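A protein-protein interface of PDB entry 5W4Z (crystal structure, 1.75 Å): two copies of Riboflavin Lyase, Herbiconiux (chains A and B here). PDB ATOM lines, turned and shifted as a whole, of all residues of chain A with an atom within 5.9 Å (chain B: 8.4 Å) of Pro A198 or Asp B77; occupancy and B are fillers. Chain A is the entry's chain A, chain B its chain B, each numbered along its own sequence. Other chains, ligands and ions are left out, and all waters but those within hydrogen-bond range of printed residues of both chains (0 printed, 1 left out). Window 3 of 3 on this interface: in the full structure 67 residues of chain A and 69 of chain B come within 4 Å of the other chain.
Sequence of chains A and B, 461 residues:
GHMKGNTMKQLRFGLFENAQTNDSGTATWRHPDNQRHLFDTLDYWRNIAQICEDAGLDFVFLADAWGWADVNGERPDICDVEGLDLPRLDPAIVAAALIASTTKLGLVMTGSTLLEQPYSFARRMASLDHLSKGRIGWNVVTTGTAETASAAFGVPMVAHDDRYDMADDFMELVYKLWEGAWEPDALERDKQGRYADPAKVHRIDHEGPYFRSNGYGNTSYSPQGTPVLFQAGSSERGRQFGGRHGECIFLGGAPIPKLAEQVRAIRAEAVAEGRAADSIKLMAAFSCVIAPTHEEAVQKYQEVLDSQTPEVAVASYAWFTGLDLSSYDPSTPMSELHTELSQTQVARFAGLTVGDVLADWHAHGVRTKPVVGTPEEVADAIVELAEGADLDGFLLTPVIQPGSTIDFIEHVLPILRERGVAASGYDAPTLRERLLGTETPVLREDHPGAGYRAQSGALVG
Among the printed residues, pairs that only touch across the chains: Val A201 with Asp B80 (3.5 Å), Pro A198 with Asp B77 (3.6 Å), Pro A198 with Asp B80 (3.6 Å), Ala A196 with Val B81 (3.8 Å), Arg A194 with Val B81 (3.8 Å) and Val A201 with Arg B75 (3.9 Å).
O of Asp B80 lies within hydrogen-bond range of N of Ala A196 (2.9 Å).
No position is printed for both chains.
NH2 of Arg A194 is in salt-bridge range of OD2 of Asp A197. The side-chain carboxylate of Asp B80 is in salt-bridge range of the guanidinium group of Arg B75 (2.8 Å). NH2 of Arg B75 lies within salt-bridge range of OD1 of Asp B85.
Of chain A, only Pro A198 (3.6 Å) comes within 4 Å of Asp B77. No residue of chain B comes within 4 Å of Ala A199. Of the printed residues of chain A, Val B81 touches Arg A194 and Ala A196. Of the printed residues of chain B, Arg A194 touches Val B81. Printed residues of chain B within 4 Å of Val A201: Arg B75 (3.9 Å) and Asp B80 (3.5 Å). The nearest residue of chain B that does not touch Pro A198 is Val B81 (4.2 Å). The nearest residue of chain A that does not touch Asp B77 is Ala A199 (5.8 Å). The nearest printed residue of chain B that does not touch Arg A194 is Asp B80 (5.1 Å).
Hydrophobic or aromatic side chains of chain A within 4 Å of the printed part of chain B: Ala A196, Pro A198 and Val A201. Among the printed residues, no Asp or Glu carboxylate lies within 4 Å of a Lys or Arg side-chain nitrogen of the other chain.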
ATOM      1  N   ARG A 194       2.201 -22.271 -28.474  1.00  0.00           N
ATOM      2  CA  ARG A 194       2.450 -21.845 -27.105  1.00  0.00           C
ATOM      3  C   ARG A 194       3.530 -22.706 -26.479  1.00  0.00           C
ATOM      4  O   ARG A 194       3.666 -23.893 -26.800  1.00  0.00           O
ATOM      5  CB  ARG A 194       1.199 -21.956 -26.230  1.00  0.00           C
ATOM      6  CG  ARG A 194       0.059 -21.059 -26.636  1.00  0.00           C
ATOM      7  CD  ARG A 194      -1.136 -21.257 -25.712  1.00  0.00           C
ATOM      8  NE  ARG A 194      -1.569 -22.652 -25.634  1.00  0.00           N
ATOM      9  CZ  ARG A 194      -2.819 -23.020 -25.363  1.00  0.00           C
ATOM     10  NH1 ARG A 194      -3.745 -22.095 -25.157  1.00  0.00           N
ATOM     11  NH2 ARG A 194      -3.151 -24.305 -25.311  1.00  0.00           N
ATOM     12  N   ALA A 196       3.384 -23.115 -23.050  1.00  0.00           N
ATOM     13  CA  ALA A 196       2.517 -23.808 -22.109  1.00  0.00           C
ATOM     14  C   ALA A 196       1.126 -23.202 -22.191  1.00  0.00           C
ATOM     15  O   ALA A 196       0.948 -22.056 -22.602  1.00  0.00           O
ATOM     16  CB  ALA A 196       3.047 -23.741 -20.668  1.00  0.00           C
ATOM     17  N   ASP A 197       0.135 -23.996 -21.826  1.00  0.00           N
ATOM     18  CA  ASP A 197      -1.251 -23.545 -21.804  1.00  0.00           C
ATOM     19  C   ASP A 197      -1.506 -22.827 -20.482  1.00  0.00           C
ATOM     20  O   ASP A 197      -1.465 -23.470 -19.426  1.00  0.00           O
ATOM     21  CB  ASP A 197      -2.172 -24.759 -21.974  1.00  0.00           C
ATOM     22  CG  ASP A 197      -3.645 -24.399 -22.036  1.00  0.00           C
ATOM     23  OD1 ASP A 197      -4.025 -23.233 -21.777  1.00  0.00           O
ATOM     24  OD2 ASP A 197      -4.433 -25.326 -22.334  1.00  0.00           O
ATOM     25  N   PRO A 198      -1.744 -21.508 -20.479  1.00  0.00           N
ATOM     26  CA  PRO A 198      -1.938 -20.818 -19.190  1.00  0.00           C
ATOM     27  C   PRO A 198      -3.097 -21.366 -18.365  1.00  0.00           C
ATOM     28  O   PRO A 198      -3.059 -21.282 -17.132  1.00  0.00           O
ATOM     29  CB  PRO A 198      -2.176 -19.357 -19.598  1.00  0.00           C
ATOM     30  CG  PRO A 198      -2.467 -19.380 -21.058  1.00  0.00           C
ATOM     31  CD  PRO A 198      -1.779 -20.576 -21.618  1.00  0.00           C
ATOM     32  N   ALA A 199      -4.120 -21.929 -19.002  1.00  0.00           N
ATOM     33  CA  ALA A 199      -5.257 -22.485 -18.272  1.00  0.00           C
ATOM     34  C   ALA A 199      -4.910 -23.743 -17.474  1.00  0.00           C
ATOM     35  O   ALA A 199      -5.698 -24.146 -16.611  1.00  0.00           O
ATOM     36  CB  ALA A 199      -6.389 -22.782 -19.257  1.00  0.00           C
ATOM     37  N   LYS A 200      -3.759 -24.365 -17.727  1.00  0.00           N
ATOM     38  CA  LYS A 200      -3.337 -25.585 -17.040  1.00  0.00           C
ATOM     39  C   LYS A 200      -2.220 -25.345 -16.029  1.00  0.00           C
ATOM     40  O   LYS A 200      -1.632 -26.302 -15.529  1.00  0.00           O
ATOM     41  CB  LYS A 200      -2.891 -26.631 -18.062  1.00  0.00           C
ATOM     42  CG  LYS A 200      -4.021 -27.081 -18.971  1.00  0.00           C
ATOM     43  CD  LYS A 200      -3.591 -28.182 -19.925  1.00  0.00           C
ATOM     44  CE  LYS A 200      -4.795 -28.726 -20.698  1.00  0.00           C
ATOM     45  NZ  LYS A 200      -4.551 -28.661 -22.169  1.00  0.00           N
ATOM     46  N   VAL A 201      -1.888 -24.090 -15.746  1.00  0.00           N
ATOM     47  CA  VAL A 201      -0.889 -23.737 -14.741  1.00  0.00           C
ATOM     48  C   VAL A 201      -1.635 -22.986 -13.646  1.00  0.00           C
ATOM     49  O   VAL A 201      -2.259 -21.954 -13.921  1.00  0.00           O
ATOM     50  CB  VAL A 201       0.233 -22.869 -15.340  1.00  0.00           C
ATOM     51  CG1 VAL A 201       1.377 -22.687 -14.335  1.00  0.00           C
ATOM     52  CG2 VAL A 201       0.730 -23.468 -16.651  1.00  0.00           C
ATOM     53  N   HIS A 202      -1.572 -23.491 -12.416  1.00  0.00           N
ATOM     54  CA  HIS A 202      -2.441 -23.016 -11.347  1.00  0.00           C
ATOM     55  C   HIS A 202      -1.656 -22.468 -10.165  1.00  0.00           C
ATOM     56  O   HIS A 202      -0.619 -23.015  -9.782  1.00  0.00           O
ATOM     57  CB  HIS A 202      -3.345 -24.150 -10.882  1.00  0.00           C
ATOM     58  CG  HIS A 202      -4.160 -24.729 -11.990  1.00  0.00           C
ATOM     59  ND1 HIS A 202      -5.231 -24.063 -12.546  1.00  0.00           N
ATOM     60  CD2 HIS A 202      -4.027 -25.880 -12.689  1.00  0.00           C
ATOM     61  CE1 HIS A 202      -5.743 -24.795 -13.519  1.00  0.00           C
ATOM     62  NE2 HIS A 202      -5.031 -25.902 -13.625  1.00  0.00           N
ATOM     63  N   ALA B  69       6.978 -14.242 -12.125  1.00  0.00           N
ATOM     64  CA  ALA B  69       6.644 -12.910 -12.637  1.00  0.00           C
ATOM     65  C   ALA B  69       5.238 -12.537 -12.182  1.00  0.00           C
ATOM     66  O   ALA B  69       4.257 -12.713 -12.905  1.00  0.00           O
ATOM     67  CB  ALA B  69       6.768 -12.870 -14.157  1.00  0.00           C
ATOM     68  N   GLU B  74      -0.946 -10.754  -9.867  1.00  0.00           N
ATOM     69  CA  GLU B  74      -1.181 -11.970 -10.632  1.00  0.00           C
ATOM     70  C   GLU B  74      -0.134 -12.119 -11.731  1.00  0.00           C
ATOM     71  O   GLU B  74       0.560 -11.174 -12.118  1.00  0.00           O
ATOM     72  CB  GLU B  74      -2.606 -12.017 -11.226  1.00  0.00           C
ATOM     73  CG  GLU B  74      -3.021 -13.370 -11.881  1.00  0.00           C
ATOM     74  CD  GLU B  74      -2.863 -14.594 -10.969  1.00  0.00           C
ATOM     75  OE1 GLU B  74      -3.884 -15.117 -10.472  1.00  0.00           O
ATOM     76  OE2 GLU B  74      -1.720 -15.050 -10.758  1.00  0.00           O
ATOM     77  N   ARG B  75      -0.029 -13.341 -12.214  1.00  0.00           N
ATOM     78  CA  ARG B  75       0.943 -13.736 -13.213  1.00  0.00           C
ATOM     79  C   ARG B  75       0.265 -13.733 -14.573  1.00  0.00           C
ATOM     80  O   ARG B  75      -0.640 -14.550 -14.800  1.00  0.00           O
ATOM     81  CB  ARG B  75       1.459 -15.120 -12.867  1.00  0.00           C
ATOM     82  CG  ARG B  75       2.605 -15.625 -13.696  1.00  0.00           C
ATOM     83  CD  ARG B  75       3.179 -16.909 -13.104  1.00  0.00           C
ATOM     84  NE  ARG B  75       4.080 -17.530 -14.064  1.00  0.00           N
ATOM     85  CZ  ARG B  75       3.719 -18.490 -14.911  1.00  0.00           C
ATOM     86  NH1 ARG B  75       2.483 -18.980 -14.876  1.00  0.00           N
ATOM     87  NH2 ARG B  75       4.601 -18.966 -15.779  1.00  0.00           N
ATOM     88  N   PRO B  76       0.629 -12.836 -15.489  1.00  0.00           N
ATOM     89  CA  PRO B  76      -0.130 -12.727 -16.741  1.00  0.00           C
ATOM     90  C   PRO B  76       0.089 -13.927 -17.652  1.00  0.00           C
ATOM     91  O   PRO B  76       1.130 -14.592 -17.613  1.00  0.00           O
ATOM     92  CB  PRO B  76       0.401 -11.435 -17.377  1.00  0.00           C
ATOM     93  CG  PRO B  76       1.709 -11.181 -16.729  1.00  0.00           C
ATOM     94  CD  PRO B  76       1.640 -11.775 -15.350  1.00  0.00           C
ATOM     95  N   ASP B  77      -0.914 -14.182 -18.501  1.00  0.00           N
ATOM     96  CA  ASP B  77      -0.924 -15.402 -19.309  1.00  0.00           C
ATOM     97  C   ASP B  77       0.290 -15.504 -20.221  1.00  0.00           C
ATOM     98  O   ASP B  77       0.728 -16.617 -20.546  1.00  0.00           O
ATOM     99  CB  ASP B  77      -2.204 -15.472 -20.136  1.00  0.00           C
ATOM    100  CG  ASP B  77      -3.412 -15.907 -19.315  1.00  0.00           C
ATOM    101  OD1 ASP B  77      -3.245 -16.282 -18.130  1.00  0.00           O
ATOM    102  OD2 ASP B  77      -4.527 -15.891 -19.872  1.00  0.00           O
ATOM    103  N   ILE B  78       0.863 -14.367 -20.625  1.00  0.00           N
ATOM    104  CA  ILE B  78       1.998 -14.388 -21.538  1.00  0.00           C
ATOM    105  C   ILE B  78       3.171 -15.153 -20.935  1.00  0.00           C
ATOM    106  O   ILE B  78       3.991 -15.731 -21.665  1.00  0.00           O
ATOM    107  CB  ILE B  78       2.372 -12.938 -21.919  1.00  0.00           C
ATOM    108  CG1 ILE B  78       3.444 -12.913 -23.005  1.00  0.00           C
ATOM    109  CG2 ILE B  78       2.810 -12.139 -20.693  1.00  0.00           C
ATOM    110  CD1 ILE B  78       2.903 -13.208 -24.378  1.00  0.00           C
ATOM    111  N   CYS B  79       3.253 -15.212 -19.601  1.00  0.00           N
ATOM    112  CA  CYS B  79       4.359 -15.912 -18.957  1.00  0.00           C
ATOM    113  C   CYS B  79       4.357 -17.400 -19.300  1.00  0.00           C
ATOM    114  O   CYS B  79       5.419 -18.017 -19.412  1.00  0.00           O
ATOM    115  CB  CYS B  79       4.299 -15.721 -17.444  1.00  0.00           C
ATOM    116  SG  CYS B  79       4.568 -14.014 -16.902  1.00  0.00           S
ATOM    117  N   ASP B  80       3.174 -17.996 -19.441  1.00  0.00           N
ATOM    118  CA  ASP B  80       3.086 -19.396 -19.841  1.00  0.00           C
ATOM    119  C   ASP B  80       3.160 -19.550 -21.356  1.00  0.00           C
ATOM    120  O   ASP B  80       3.815 -20.474 -21.851  1.00  0.00           O
ATOM    121  CB  ASP B  80       1.802 -20.015 -19.280  1.00  0.00           C
ATOM    122  CG  ASP B  80       1.863 -20.171 -17.767  1.00  0.00           C
ATOM    123  OD1 ASP B  80       2.925 -20.612 -17.271  1.00  0.00           O
ATOM    124  OD2 ASP B  80       0.873 -19.844 -17.080  1.00  0.00           O
ATOM    125  N   VAL B  81       2.542 -18.639 -22.108  1.00  0.00           N
ATOM    126  CA  VAL B  81       2.625 -18.708 -23.566  1.00  0.00           C
ATOM    127  C   VAL B  81       4.077 -18.648 -24.025  1.00  0.00           C
ATOM    128  O   VAL B  81       4.463 -19.310 -24.994  1.00  0.00           O
ATOM    129  CB  VAL B  81       1.776 -17.593 -24.208  1.00  0.00           C
ATOM    130  CG1 VAL B  81       2.040 -17.514 -25.705  1.00  0.00           C
ATOM    131  CG2 VAL B  81       0.292 -17.834 -23.949  1.00  0.00           C
ATOM    132  N   GLU B  82       4.911 -17.868 -23.331  1.00  0.00           N
ATOM    133  CA  GLU B  82       6.307 -17.705 -23.712  1.00  0.00           C
ATOM    134  C   GLU B  82       7.283 -18.406 -22.779  1.00  0.00           C
ATOM    135  O   GLU B  82       8.494 -18.314 -23.007  1.00  0.00           O
ATOM    136  CB  GLU B  82       6.660 -16.209 -23.793  1.00  0.00           C
ATOM    137  CG  GLU B  82       5.801 -15.449 -24.784  1.00  0.00           C
ATOM    138  CD  GLU B  82       5.989 -15.907 -26.225  1.00  0.00           C
ATOM    139  OE1 GLU B  82       7.093 -16.397 -26.582  1.00  0.00           O
ATOM    140  OE2 GLU B  82       5.025 -15.754 -26.999  1.00  0.00           O
ATOM    141  N   GLY B  83       6.812 -19.132 -21.768  1.00  0.00           N
ATOM    142  CA  GLY B  83       7.768 -19.806 -20.887  1.00  0.00           C
ATOM    143  C   GLY B  83       8.773 -18.838 -20.301  1.00  0.00           C
ATOM    144  O   GLY B  83       9.973 -19.135 -20.211  1.00  0.00           O
ATOM    145  N   LEU B  84       8.296 -17.655 -19.933  1.00  0.00           N
ATOM    146  CA  LEU B  84       9.174 -16.569 -19.511  1.00  0.00           C
ATOM    147  C   LEU B  84       9.944 -16.933 -18.249  1.00  0.00           C
ATOM    148  O   LEU B  84      11.177 -16.821 -18.203  1.00  0.00           O
ATOM    149  CB  LEU B  84       8.332 -15.321 -19.282  1.00  0.00           C
ATOM    150  CG  LEU B  84       9.125 -14.100 -18.826  1.00  0.00           C
ATOM    151  CD1 LEU B  84      10.217 -13.760 -19.837  1.00  0.00           C
ATOM    152  CD2 LEU B  84       8.179 -12.946 -18.620  1.00  0.00           C
ATOM    153  N   ASP B  85       9.230 -17.387 -17.216  1.00  0.00           N
ATOM    154  CA  ASP B  85       9.774 -17.491 -15.869  1.00  0.00           C
ATOM    155  C   ASP B  85       9.771 -18.897 -15.309  1.00  0.00           C
ATOM    156  O   ASP B  85      10.620 -19.211 -14.467  1.00  0.00           O
ATOM    157  CB  ASP B  85       8.976 -16.586 -14.908  1.00  0.00           C
ATOM    158  CG  ASP B  85       7.473 -16.863 -14.930  1.00  0.00           C
ATOM    159  OD1 ASP B  85       6.959 -17.479 -15.892  1.00  0.00           O
ATOM    160  OD2 ASP B  85       6.789 -16.435 -13.973  1.00  0.00           O
ATOM    161  N   GLU B 311       5.955  -8.354 -25.941  1.00  0.00           N
ATOM    162  CA  GLU B 311       4.890  -8.414 -24.948  1.00  0.00           C
ATOM    163  C   GLU B 311       5.351  -8.970 -23.607  1.00  0.00           C
ATOM    164  O   GLU B 311       4.623  -8.818 -22.620  1.00  0.00           O
ATOM    165  CB  GLU B 311       3.736  -9.251 -25.492  1.00  0.00           C
ATOM    166  CG  GLU B 311       3.316  -8.842 -26.893  1.00  0.00           C
ATOM    167  CD  GLU B 311       2.071  -9.561 -27.367  1.00  0.00           C
ATOM    168  OE1 GLU B 311       1.594 -10.472 -26.654  1.00  0.00           O
ATOM    169  OE2 GLU B 311       1.566  -9.209 -28.455  1.00  0.00           O
ATOM    170  N   ALA B 315       5.963  -8.102 -17.545  1.00  0.00           N
ATOM    171  CA  ALA B 315       6.063  -9.187 -16.572  1.00  0.00           C
ATOM    172  C   ALA B 315       7.521  -9.505 -16.272  1.00  0.00           C
ATOM    173  O   ALA B 315       7.888  -9.763 -15.117  1.00  0.00           O
ATOM    174  CB  ALA B 315       5.329 -10.426 -17.087  1.00  0.00           C
